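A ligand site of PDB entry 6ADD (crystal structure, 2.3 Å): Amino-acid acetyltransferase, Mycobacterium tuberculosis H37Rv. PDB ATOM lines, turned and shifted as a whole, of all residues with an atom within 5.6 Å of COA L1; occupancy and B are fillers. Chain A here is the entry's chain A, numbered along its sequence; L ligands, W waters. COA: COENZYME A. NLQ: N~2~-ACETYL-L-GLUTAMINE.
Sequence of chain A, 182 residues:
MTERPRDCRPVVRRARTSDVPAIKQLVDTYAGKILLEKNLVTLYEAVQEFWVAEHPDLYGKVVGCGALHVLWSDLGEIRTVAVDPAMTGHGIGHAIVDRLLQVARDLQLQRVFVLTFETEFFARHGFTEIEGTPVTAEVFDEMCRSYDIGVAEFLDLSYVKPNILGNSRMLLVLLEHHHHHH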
ATOM      1  N   ASP A   7     -12.108 -23.155  -2.790  1.00  0.00           N
ATOM      2  CA  ASP A   7     -11.325 -23.039  -4.020  1.00  0.00           C
ATOM      3  C   ASP A   7      -9.835 -22.857  -3.705  1.00  0.00           C
ATOM      4  O   ASP A   7      -9.470 -22.283  -2.675  1.00  0.00           O
ATOM      5  CB  ASP A   7     -11.827 -21.875  -4.886  1.00  0.00           C
ATOM      6  CG  ASP A   7     -13.142 -22.193  -5.595  1.00  0.00           C
ATOM      7  OD1 ASP A   7     -13.767 -23.226  -5.291  1.00  0.00           O
ATOM      8  OD2 ASP A   7     -13.554 -21.404  -6.478  1.00  0.00           O
ATOM      9  N   CYS A   8      -8.982 -23.355  -4.600  1.00  0.00           N
ATOM     10  CA  CYS A   8      -7.550 -23.315  -4.377  1.00  0.00           C
ATOM     11  C   CYS A   8      -6.975 -21.962  -4.789  1.00  0.00           C
ATOM     12  O   CYS A   8      -7.529 -21.250  -5.640  1.00  0.00           O
ATOM     13  CB  CYS A   8      -6.850 -24.423  -5.148  1.00  0.00           C
ATOM     14  SG  CYS A   8      -6.571 -24.031  -6.901  1.00  0.00           S
ATOM     15  N   TYR A  30     -15.220  -2.214 -14.993  1.00  0.00           N
ATOM     16  CA  TYR A  30     -15.471  -1.390 -13.818  1.00  0.00           C
ATOM     17  C   TYR A  30     -15.095   0.068 -14.000  1.00  0.00           C
ATOM     18  O   TYR A  30     -15.150   0.833 -13.034  1.00  0.00           O
ATOM     19  CB  TYR A  30     -14.700  -1.975 -12.631  1.00  0.00           C
ATOM     20  CG  TYR A  30     -15.014  -3.416 -12.316  1.00  0.00           C
ATOM     21  CD1 TYR A  30     -16.191  -3.760 -11.637  1.00  0.00           C
ATOM     22  CD2 TYR A  30     -14.142  -4.429 -12.668  1.00  0.00           C
ATOM     23  CE1 TYR A  30     -16.478  -5.084 -11.342  1.00  0.00           C
ATOM     24  CE2 TYR A  30     -14.422  -5.741 -12.370  1.00  0.00           C
ATOM     25  CZ  TYR A  30     -15.588  -6.077 -11.709  1.00  0.00           C
ATOM     26  OH  TYR A  30     -15.852  -7.403 -11.423  1.00  0.00           O
ATOM     27  N   ILE A  34     -15.948   3.221 -10.290  1.00  0.00           N
ATOM     28  CA  ILE A  34     -15.157   2.279  -9.502  1.00  0.00           C
ATOM     29  C   ILE A  34     -13.666   2.386  -9.858  1.00  0.00           C
ATOM     30  O   ILE A  34     -12.832   2.735  -9.009  1.00  0.00           O
ATOM     31  CB  ILE A  34     -15.675   0.841  -9.697  1.00  0.00           C
ATOM     32  CG1 ILE A  34     -17.129   0.721  -9.198  1.00  0.00           C
ATOM     33  CG2 ILE A  34     -14.770  -0.151  -8.977  1.00  0.00           C
ATOM     34  CD1 ILE A  34     -17.772  -0.646  -9.434  1.00  0.00           C
ATOM     35  N   LEU A  35     -13.303   2.097 -11.106  1.00  0.00           N
ATOM     36  CA  LEU A  35     -11.907   2.106 -11.514  1.00  0.00           C
ATOM     37  C   LEU A  35     -11.608   3.309 -12.408  1.00  0.00           C
ATOM     38  O   LEU A  35     -12.427   3.721 -13.228  1.00  0.00           O
ATOM     39  CB  LEU A  35     -11.523   0.822 -12.248  1.00  0.00           C
ATOM     40  CG  LEU A  35     -11.416  -0.454 -11.397  1.00  0.00           C
ATOM     41  CD1 LEU A  35     -10.852  -1.619 -12.212  1.00  0.00           C
ATOM     42  CD2 LEU A  35     -10.605  -0.242 -10.128  1.00  0.00           C
ATOM     43  N   ILE A  78      -1.654   0.369  -4.307  1.00  0.00           N
ATOM     44  CA  ILE A  78      -2.361  -0.695  -4.998  1.00  0.00           C
ATOM     45  C   ILE A  78      -3.422  -0.056  -5.882  1.00  0.00           C
ATOM     46  O   ILE A  78      -4.206   0.782  -5.412  1.00  0.00           O
ATOM     47  CB  ILE A  78      -2.973  -1.688  -3.990  1.00  0.00           C
ATOM     48  CG1 ILE A  78      -1.864  -2.555  -3.390  1.00  0.00           C
ATOM     49  CG2 ILE A  78      -4.015  -2.568  -4.669  1.00  0.00           C
ATOM     50  CD1 ILE A  78      -2.379  -3.550  -2.406  1.00  0.00           C
ATOM     51  N   ARG A  79      -3.426  -0.390  -7.167  1.00  0.00           N
ATOM     52  CA  ARG A  79      -4.349   0.224  -8.108  1.00  0.00           C
ATOM     53  C   ARG A  79      -4.761  -0.807  -9.144  1.00  0.00           C
ATOM     54  O   ARG A  79      -4.054  -1.791  -9.397  1.00  0.00           O
ATOM     55  CB  ARG A  79      -3.733   1.462  -8.795  1.00  0.00           C
ATOM     56  CG  ARG A  79      -2.439   1.141  -9.584  1.00  0.00           C
ATOM     57  CD  ARG A  79      -2.066   2.217 -10.577  1.00  0.00           C
ATOM     58  NE  ARG A  79      -1.787   3.509  -9.940  1.00  0.00           N
ATOM     59  CZ  ARG A  79      -1.400   4.604 -10.596  1.00  0.00           C
ATOM     60  NH1 ARG A  79      -1.215   4.584 -11.922  1.00  0.00           N
ATOM     61  NH2 ARG A  79      -1.214   5.733  -9.913  1.00  0.00           N
ATOM     62  N   THR A  80      -5.922  -0.557  -9.750  1.00  0.00           N
ATOM     63  CA  THR A  80      -6.359  -1.321 -10.915  1.00  0.00           C
ATOM     64  C   THR A  80      -6.477  -2.809 -10.588  1.00  0.00           C
ATOM     65  O   THR A  80      -6.023  -3.664 -11.354  1.00  0.00           O
ATOM     66  CB  THR A  80      -5.412  -1.087 -12.104  1.00  0.00           C
ATOM     67  OG1 THR A  80      -4.948   0.283 -12.085  1.00  0.00           O
ATOM     68  CG2 THR A  80      -6.151  -1.326 -13.405  1.00  0.00           C
ATOM     69  N   VAL A  81      -7.048  -3.125  -9.436  1.00  0.00           N
ATOM     70  CA  VAL A  81      -7.393  -4.498  -9.085  1.00  0.00           C
ATOM     71  C   VAL A  81      -8.776  -4.784  -9.647  1.00  0.00           C
ATOM     72  O   VAL A  81      -9.723  -4.046  -9.339  1.00  0.00           O
ATOM     73  CB  VAL A  81      -7.347  -4.739  -7.561  1.00  0.00           C
ATOM     74  CG1 VAL A  81      -7.751  -6.194  -7.245  1.00  0.00           C
ATOM     75  CG2 VAL A  81      -5.966  -4.441  -7.007  1.00  0.00           C
ATOM     76  N   ALA A  82      -8.885  -5.804 -10.482  1.00  0.00           N
ATOM     77  CA  ALA A  82     -10.167  -6.135 -11.100  1.00  0.00           C
ATOM     78  C   ALA A  82     -10.257  -7.646 -11.273  1.00  0.00           C
ATOM     79  O   ALA A  82      -9.305  -8.288 -11.712  1.00  0.00           O
ATOM     80  CB  ALA A  82     -10.317  -5.449 -12.466  1.00  0.00           C
ATOM     81  N   VAL A  83     -11.421  -8.198 -10.956  1.00  0.00           N
ATOM     82  CA  VAL A  83     -11.701  -9.618 -11.099  1.00  0.00           C
ATOM     83  C   VAL A  83     -12.917  -9.770 -11.997  1.00  0.00           C
ATOM     84  O   VAL A  83     -13.859  -8.982 -11.893  1.00  0.00           O
ATOM     85  CB  VAL A  83     -11.933 -10.270  -9.719  1.00  0.00           C
ATOM     86  CG1 VAL A  83     -12.438 -11.707  -9.861  1.00  0.00           C
ATOM     87  CG2 VAL A  83     -10.649 -10.241  -8.899  1.00  0.00           C
ATOM     88  N   MET A  87     -16.462 -14.474 -11.681  1.00  0.00           N
ATOM     89  CA  MET A  87     -15.502 -15.280 -10.920  1.00  0.00           C
ATOM     90  C   MET A  87     -15.214 -14.699  -9.552  1.00  0.00           C
ATOM     91  O   MET A  87     -14.304 -15.162  -8.863  1.00  0.00           O
ATOM     92  CB  MET A  87     -14.190 -15.419 -11.692  1.00  0.00           C
ATOM     93  CG  MET A  87     -14.322 -16.056 -13.052  1.00  0.00           C
ATOM     94  SD  MET A  87     -14.642 -17.818 -12.912  1.00  0.00           S
ATOM     95  CE  MET A  87     -13.035 -18.415 -12.404  1.00  0.00           C
ATOM     96  N   THR A  88     -15.979 -13.695  -9.133  1.00  0.00           N
ATOM     97  CA  THR A  88     -15.761 -13.084  -7.835  1.00  0.00           C
ATOM     98  C   THR A  88     -16.190 -14.034  -6.721  1.00  0.00           C
ATOM     99  O   THR A  88     -16.928 -15.006  -6.936  1.00  0.00           O
ATOM    100  CB  THR A  88     -16.544 -11.773  -7.752  1.00  0.00           C
ATOM    101  OG1 THR A  88     -17.877 -11.999  -8.243  1.00  0.00           O
ATOM    102  CG2 THR A  88     -15.877 -10.706  -8.604  1.00  0.00           C
ATOM    103  N   GLY A  89     -15.748 -13.716  -5.503  1.00  0.00           N
ATOM    104  CA  GLY A  89     -16.090 -14.525  -4.346  1.00  0.00           C
ATOM    105  C   GLY A  89     -15.446 -15.896  -4.288  1.00  0.00           C
ATOM    106  O   GLY A  89     -16.012 -16.813  -3.692  1.00  0.00           O
ATOM    107  N   HIS A  90     -14.287 -16.076  -4.926  1.00  0.00           N
ATOM    108  CA  HIS A  90     -13.577 -17.346  -4.910  1.00  0.00           C
ATOM    109  C   HIS A  90     -12.128 -17.215  -4.425  1.00  0.00           C
ATOM    110  O   HIS A  90     -11.349 -18.160  -4.580  1.00  0.00           O
ATOM    111  CB  HIS A  90     -13.600 -17.990  -6.296  1.00  0.00           C
ATOM    112  CG  HIS A  90     -14.936 -18.509  -6.717  1.00  0.00           C
ATOM    113  ND1 HIS A  90     -15.523 -19.623  -6.162  1.00  0.00           N
ATOM    114  CD2 HIS A  90     -15.810 -18.062  -7.656  1.00  0.00           C
ATOM    115  CE1 HIS A  90     -16.690 -19.849  -6.734  1.00  0.00           C
ATOM    116  NE2 HIS A  90     -16.885 -18.911  -7.647  1.00  0.00           N
ATOM    117  N   GLY A  91     -11.744 -16.067  -3.869  1.00  0.00           N
ATOM    118  CA  GLY A  91     -10.392 -15.836  -3.375  1.00  0.00           C
ATOM    119  C   GLY A  91      -9.411 -15.198  -4.355  1.00  0.00           C
ATOM    120  O   GLY A  91      -8.240 -15.007  -3.987  1.00  0.00           O
ATOM    121  N   ILE A  92      -9.848 -14.839  -5.556  1.00  0.00           N
ATOM    122  CA  ILE A  92      -8.915 -14.333  -6.562  1.00  0.00           C
ATOM    123  C   ILE A  92      -8.466 -12.908  -6.210  1.00  0.00           C
ATOM    124  O   ILE A  92      -7.282 -12.580  -6.272  1.00  0.00           O
ATOM    125  CB  ILE A  92      -9.554 -14.416  -7.961  1.00  0.00           C
ATOM    126  CG1 ILE A  92      -9.773 -15.879  -8.348  1.00  0.00           C
ATOM    127  CG2 ILE A  92      -8.668 -13.691  -9.008  1.00  0.00           C
ATOM    128  CD1 ILE A  92     -10.709 -16.088  -9.542  1.00  0.00           C
ATOM    129  N   GLY A  93      -9.423 -12.046  -5.809  1.00  0.00           N
ATOM    130  CA  GLY A  93      -9.057 -10.701  -5.390  1.00  0.00           C
ATOM    131  C   GLY A  93      -8.023 -10.689  -4.281  1.00  0.00           C
ATOM    132  O   GLY A  93      -7.003  -9.994  -4.375  1.00  0.00           O
ATOM    133  N   HIS A  94      -8.280 -11.453  -3.221  1.00  0.00           N
ATOM    134  CA  HIS A  94      -7.327 -11.497  -2.101  1.00  0.00           C
ATOM    135  C   HIS A  94      -5.978 -12.084  -2.509  1.00  0.00           C
ATOM    136  O   HIS A  94      -4.944 -11.655  -1.997  1.00  0.00           O
ATOM    137  CB  HIS A  94      -7.922 -12.287  -0.947  1.00  0.00           C
ATOM    138  CG  HIS A  94      -8.989 -11.549  -0.192  1.00  0.00           C
ATOM    139  ND1 HIS A  94      -8.761 -10.317   0.375  1.00  0.00           N
ATOM    140  CD2 HIS A  94     -10.274 -11.866   0.073  1.00  0.00           C
ATOM    141  CE1 HIS A  94      -9.875  -9.901   0.962  1.00  0.00           C
ATOM    142  NE2 HIS A  94     -10.808 -10.818   0.788  1.00  0.00           N
ATOM    143  N   ALA A  95      -5.973 -13.066  -3.420  1.00  0.00           N
ATOM    144  CA  ALA A  95      -4.689 -13.636  -3.838  1.00  0.00           C
ATOM    145  C   ALA A  95      -3.855 -12.619  -4.607  1.00  0.00           C
ATOM    146  O   ALA A  95      -2.632 -12.600  -4.487  1.00  0.00           O
ATOM    147  CB  ALA A  95      -4.916 -14.898  -4.681  1.00  0.00           C
ATOM    148  N   VAL A 114      -4.358   2.856  -0.925  1.00  0.00           N
ATOM    149  CA  VAL A 114      -5.383   2.446  -1.865  1.00  0.00           C
ATOM    150  C   VAL A 114      -6.576   3.388  -1.708  1.00  0.00           C
ATOM    151  O   VAL A 114      -6.913   3.824  -0.607  1.00  0.00           O
ATOM    152  CB  VAL A 114      -5.784   0.957  -1.672  1.00  0.00           C
ATOM    153  CG1 VAL A 114      -6.323   0.715  -0.261  1.00  0.00           C
ATOM    154  CG2 VAL A 114      -6.786   0.520  -2.741  1.00  0.00           C
ATOM    155  N   LEU A 115      -7.168   3.752  -2.836  1.00  0.00           N
ATOM    156  CA  LEU A 115      -8.404   4.533  -2.857  1.00  0.00           C
ATOM    157  C   LEU A 115      -9.498   3.615  -3.383  1.00  0.00           C
ATOM    158  O   LEU A 115      -9.390   3.115  -4.516  1.00  0.00           O
ATOM    159  CB  LEU A 115      -8.226   5.765  -3.741  1.00  0.00           C
ATOM    160  CG  LEU A 115      -9.333   6.815  -3.809  1.00  0.00           C
ATOM    161  CD1 LEU A 115      -9.552   7.483  -2.435  1.00  0.00           C
ATOM    162  CD2 LEU A 115      -8.966   7.858  -4.853  1.00  0.00           C
ATOM    163  N   THR A 116     -10.531   3.386  -2.582  1.00  0.00           N
ATOM    164  CA  THR A 116     -11.430   2.302  -2.951  1.00  0.00           C
ATOM    165  C   THR A 116     -12.778   2.462  -2.259  1.00  0.00           C
ATOM    166  O   THR A 116     -12.889   3.123  -1.230  1.00  0.00           O
ATOM    167  CB  THR A 116     -10.814   0.942  -2.613  1.00  0.00           C
ATOM    168  OG1 THR A 116     -11.703  -0.118  -3.027  1.00  0.00           O
ATOM    169  CG2 THR A 116     -10.529   0.843  -1.109  1.00  0.00           C
ATOM    170  N   GLU A 118     -14.173  -0.618  -1.743  1.00  0.00           N
ATOM    171  CA  GLU A 118     -14.181  -1.945  -1.119  1.00  0.00           C
ATOM    172  C   GLU A 118     -13.411  -1.893   0.199  1.00  0.00           C
ATOM    173  O   GLU A 118     -12.385  -2.538   0.395  1.00  0.00           O
ATOM    174  CB  GLU A 118     -13.587  -3.003  -2.040  1.00  0.00           C
ATOM    175  CG  GLU A 118     -14.398  -3.229  -3.291  1.00  0.00           C
ATOM    176  CD  GLU A 118     -15.726  -3.900  -3.016  1.00  0.00           C
ATOM    177  OE1 GLU A 118     -15.905  -4.453  -1.907  1.00  0.00           O
ATOM    178  OE2 GLU A 118     -16.594  -3.857  -3.902  1.00  0.00           O
ATOM    179  N   GLU A 120     -13.989  -3.121   3.228  1.00  0.00           N
ATOM    180  CA  GLU A 120     -13.801  -4.366   3.948  1.00  0.00           C
ATOM    181  C   GLU A 120     -12.836  -5.329   3.264  1.00  0.00           C
ATOM    182  O   GLU A 120     -12.067  -5.932   3.939  1.00  0.00           O
ATOM    183  CB  GLU A 120     -15.114  -5.046   4.367  1.00  0.00           C
ATOM    184  N   PHE A 121     -12.865  -5.448   1.939  1.00  0.00           N
ATOM    185  CA  PHE A 121     -11.933  -6.297   1.229  1.00  0.00           C
ATOM    186  C   PHE A 121     -10.515  -5.943   1.634  1.00  0.00           C
ATOM    187  O   PHE A 121      -9.740  -6.815   2.015  1.00  0.00           O
ATOM    188  CB  PHE A 121     -12.160  -6.141  -0.267  1.00  0.00           C
ATOM    189  CG  PHE A 121     -11.145  -6.832  -1.107  1.00  0.00           C
ATOM    190  CD1 PHE A 121     -11.278  -8.173  -1.416  1.00  0.00           C
ATOM    191  CD2 PHE A 121     -10.075  -6.135  -1.600  1.00  0.00           C
ATOM    192  CE1 PHE A 121     -10.333  -8.806  -2.215  1.00  0.00           C
ATOM    193  CE2 PHE A 121      -9.133  -6.759  -2.397  1.00  0.00           C
ATOM    194  CZ  PHE A 121      -9.259  -8.091  -2.693  1.00  0.00           C
ATOM    195  N   PHE A 122     -10.214  -4.643   1.675  1.00  0.00           N
ATOM    196  CA  PHE A 122      -8.867  -4.217   2.011  1.00  0.00           C
ATOM    197  C   PHE A 122      -8.595  -4.213   3.510  1.00  0.00           C
ATOM    198  O   PHE A 122      -7.416  -4.291   3.903  1.00  0.00           O
ATOM    199  CB  PHE A 122      -8.596  -2.839   1.419  1.00  0.00           C
ATOM    200  CG  PHE A 122      -8.339  -2.897  -0.067  1.00  0.00           C
ATOM    201  CD1 PHE A 122      -7.115  -3.310  -0.543  1.00  0.00           C
ATOM    202  CD2 PHE A 122      -9.345  -2.568  -0.974  1.00  0.00           C
ATOM    203  CE1 PHE A 122      -6.881  -3.385  -1.900  1.00  0.00           C
ATOM    204  CE2 PHE A 122      -9.114  -2.635  -2.319  1.00  0.00           C
ATOM    205  CZ  PHE A 122      -7.893  -3.038  -2.792  1.00  0.00           C
ATOM    206  N   ARG A 124      -9.266  -6.651   5.357  1.00  0.00           N
ATOM    207  CA  ARG A 124      -8.769  -7.994   5.629  1.00  0.00           C
ATOM    208  C   ARG A 124      -7.252  -8.037   5.578  1.00  0.00           C
ATOM    209  O   ARG A 124      -6.643  -8.882   6.243  1.00  0.00           O
ATOM    210  CB  ARG A 124      -9.356  -9.006   4.628  1.00  0.00           C
ATOM    211  CG  ARG A 124     -10.853  -9.235   4.776  1.00  0.00           C
ATOM    212  CD  ARG A 124     -11.181  -9.823   6.134  1.00  0.00           C
ATOM    213  NE  ARG A 124     -12.609  -9.842   6.413  1.00  0.00           N
ATOM    214  CZ  ARG A 124     -13.313  -8.808   6.865  1.00  0.00           C
ATOM    215  NH1 ARG A 124     -12.715  -7.645   7.099  1.00  0.00           N
ATOM    216  NH2 ARG A 124     -14.615  -8.939   7.083  1.00  0.00           N
HETATM  217  N1A COA L   1     -11.228 -18.574  -0.985  1.00  0.00           N
HETATM  218  C2A COA L   1     -10.975 -17.379  -0.457  1.00  0.00           C
HETATM  219  N3A COA L   1     -12.008 -16.496  -0.232  1.00  0.00           N
HETATM  220  C4A COA L   1     -13.276 -16.848  -0.523  1.00  0.00           C
HETATM  221  C5A COA L   1     -13.529 -18.044  -1.041  1.00  0.00           C
HETATM  222  C6A COA L   1     -12.493 -18.934  -1.278  1.00  0.00           C
HETATM  223  N6A COA L   1     -12.477 -20.256  -1.820  1.00  0.00           N
HETATM  224  N7A COA L   1     -14.879 -18.144  -1.232  1.00  0.00           N
HETATM  225  C8A COA L   1     -15.440 -16.988  -0.822  1.00  0.00           C
HETATM  226  N9A COA L   1     -14.450 -16.191  -0.396  1.00  0.00           N
HETATM  227  C1B COA L   1     -15.055 -14.986   0.024  1.00  0.00           C
HETATM  228  C2B COA L   1     -14.228 -14.384   0.875  1.00  0.00           C
HETATM  229  O2B COA L   1     -14.618 -14.658   2.227  1.00  0.00           O
HETATM  230  C3B COA L   1     -14.339 -12.789   0.601  1.00  0.00           C
HETATM  231  O3B COA L   1     -15.023 -12.187   1.689  1.00  0.00           O
HETATM  232  P3B COA L   1     -14.124 -11.171   2.661  1.00  0.00           P
HETATM  233  O7A COA L   1     -15.018 -10.664   3.783  1.00  0.00           O
HETATM  234  O8A COA L   1     -12.933 -11.920   3.215  1.00  0.00           O
HETATM  235  O9A COA L   1     -13.644  -9.978   1.829  1.00  0.00           O
HETATM  236  C4B COA L   1     -15.033 -12.594  -0.556  1.00  0.00           C
HETATM  237  O4B COA L   1     -15.153 -13.981  -1.196  1.00  0.00           O
HETATM  238  C5B COA L   1     -14.200 -11.672  -1.463  1.00  0.00           C
HETATM  239  O5B COA L   1     -12.894 -12.164  -1.467  1.00  0.00           O
HETATM  240  P1A COA L   1     -12.177 -12.519  -2.935  1.00  0.00           P
HETATM  241  O1A COA L   1     -12.937 -13.612  -3.648  1.00  0.00           O
HETATM  242  O2A COA L   1     -10.771 -12.941  -2.717  1.00  0.00           O
HETATM  243  O3A COA L   1     -12.174 -11.146  -3.847  1.00  0.00           O
HETATM  244  P2A COA L   1     -12.877 -11.074  -5.346  1.00  0.00           P
HETATM  245  O4A COA L   1     -12.221 -12.114  -6.227  1.00  0.00           O
HETATM  246  O5A COA L   1     -14.405 -11.300  -5.292  1.00  0.00           O
HETATM  247  O6A COA L   1     -12.620  -9.535  -5.960  1.00  0.00           O
HETATM  248  CBP COA L   1     -12.771  -7.144  -5.921  1.00  0.00           C
HETATM  249  CCP COA L   1     -12.742  -8.438  -5.080  1.00  0.00           C
HETATM  250  CDP COA L   1     -13.264  -6.032  -5.073  1.00  0.00           C
HETATM  251  CEP COA L   1     -11.369  -6.806  -6.411  1.00  0.00           C
HETATM  252  CAP COA L   1     -13.732  -7.365  -7.140  1.00  0.00           C
HETATM  253  OAP COA L   1     -15.042  -7.460  -6.676  1.00  0.00           O
HETATM  254  C9P COA L   1     -13.608  -6.238  -8.138  1.00  0.00           C
HETATM  255  O9P COA L   1     -12.909  -6.381  -9.129  1.00  0.00           O
HETATM  256  N8P COA L   1     -14.320  -4.989  -7.932  1.00  0.00           N
HETATM  257  C7P COA L   1     -14.211  -3.879  -8.872  1.00  0.00           C
HETATM  258  C6P COA L   1     -12.755  -3.278  -8.888  1.00  0.00           C
HETATM  259  C5P COA L   1     -12.371  -2.717  -7.509  1.00  0.00           C
HETATM  260  O5P COA L   1     -13.220  -2.355  -6.710  1.00  0.00           O
HETATM  261  N4P COA L   1     -10.962  -2.610  -7.146  1.00  0.00           N
HETATM  262  C3P COA L   1     -10.529  -2.058  -5.807  1.00  0.00           C
HETATM  263  C2P COA L   1      -9.850  -0.723  -6.031  1.00  0.00           C
HETATM  264  S1P COA L   1      -8.345  -0.871  -6.998  1.00  0.00           S
HETATM  265  OXT NLQ L   2      -8.919   2.450  -6.969  1.00  0.00           O
HETATM  266  C   NLQ L   2      -8.369   3.660  -7.254  1.00  0.00           C
HETATM  267  O   NLQ L   2      -7.458   4.057  -6.522  1.00  0.00           O
HETATM  268  CA  NLQ L   2      -8.969   4.369  -8.460  1.00  0.00           C
HETATM  269  N   NLQ L   2      -8.685   3.728  -9.741  1.00  0.00           N
HETATM  270  C6  NLQ L   2      -7.992   2.556 -10.022  1.00  0.00           C
HETATM  271  O4  NLQ L   2      -7.501   1.830  -9.138  1.00  0.00           O
HETATM  272  C7  NLQ L   2      -7.830   2.177 -11.472  1.00  0.00           C
HETATM  273  CB  NLQ L   2     -10.488   4.502  -8.159  1.00  0.00           C
HETATM  274  CG  NLQ L   2     -10.954   5.955  -8.142  1.00  0.00           C
HETATM  275  CD  NLQ L   2     -11.705   6.402  -9.394  1.00  0.00           C
HETATM  276  NE2 NLQ L   2     -11.116   7.284 -10.267  1.00  0.00           N
HETATM  277  OE1 NLQ L   2     -12.843   5.993  -9.701  1.00  0.00           O
HETATM  278  O   HOH W   1     -13.092   0.397  -5.236  1.00  0.00           O
HETATM  279  O   HOH W   2     -12.757 -14.667  -6.665  1.00  0.00           O
HETATM  280  O   HOH W   3     -15.999  -2.973  -6.439  1.00  0.00           O
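S1P of COA L1 sits close to N of Thr 80 (3.7 Å).
The backbone NH of His 94 lies within hydrogen-bond range of an oxygen (O2A) of COA L1 (2.9 Å).
O1A of COA L1 lies within hydrogen-bond range of N of His 90.
The backbone NH (N) of Gly 93 is in hydrogen-bond range of an oxygen (O4A) of COA L1, at 2.8 Å.
N of Gly 89 sits at hydrogen-bond distance from O5A of COA L1 (2.8 Å).
The guanidinium group (NE) of Arg 124 is in salt-bridge range of an oxygen (O7A) of COA L1.
The backbone carbonyl oxygen of Val 81 is in hydrogen-bond range of a nitrogen (N4P) of COA L1.
A ring nitrogen (NE2) of His 94 is in hydrogen-bond range of an oxygen (O9A) of COA L1.
N of Val 81 sits close to S1P of COA L1.
The backbone NH of Gly 91 sits at hydrogen-bond distance from an oxygen (O1A) of COA L1.
N of Val 83 sits at hydrogen-bond distance from O9P of COA L1, 3.0 Å away.
The backbone carbonyl oxygen (O) of Leu 115 sits close to an oxygen (OXT) of NLQ L2 (2.6 Å).
An oxygen (O4) of NLQ L2 sits at hydrogen-bond distance from the backbone NH of Thr 80 (2.9 Å).
An oxygen (OXT) of NLQ L2 lies close to a sulfur (S1P) of COA L1 (3.4 Å).
OD2 of Asp 7 lies within hydrogen-bond range of ND1 of His 90 (2.7 Å).
OG1 of Thr 116 lies within hydrogen-bond range of N of Glu 118, at 2.8 Å.
The backbone carbonyl oxygen (O) of Val 83 is in hydrogen-bond range of the side-chain hydroxyl (OH) of Tyr 30.
The backbone carbonyl oxygen (O) of Tyr 30 lies within hydrogen-bond range of the backbone NH (N) of Leu 35, at 3.0 Å.
N6A of COA L1 sits close to N of Asp 7 (3.1 Å).
Residues that only touch COA L1: Thr 88, Ala 82, Phe 121, Tyr 30, Glu 118, Ile 34, Ile 92, Thr 116, Phe 122 and Leu 35.
Hydrophobic or aromatic side chains that line COA L1: Tyr 30, Ile 34, Leu 35, Val 81, Val 83, Ile 92, His 94, Phe 121 and Phe 122.
Of the 28 residues printed, 20 come within 4 Å of COA L1.
The nearest printed residue that does not touch COA L1 is Leu 115 (4.2 Å).
Water W3 bridges the side-chain carboxylate (OE2) of Glu 118 (2.8 Å) and an oxygen (O5P) of COA L1 (2.9 Å).
Water W1 lies within hydrogen-bond range of OG1 of Thr 116 and O5P of COA L1.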
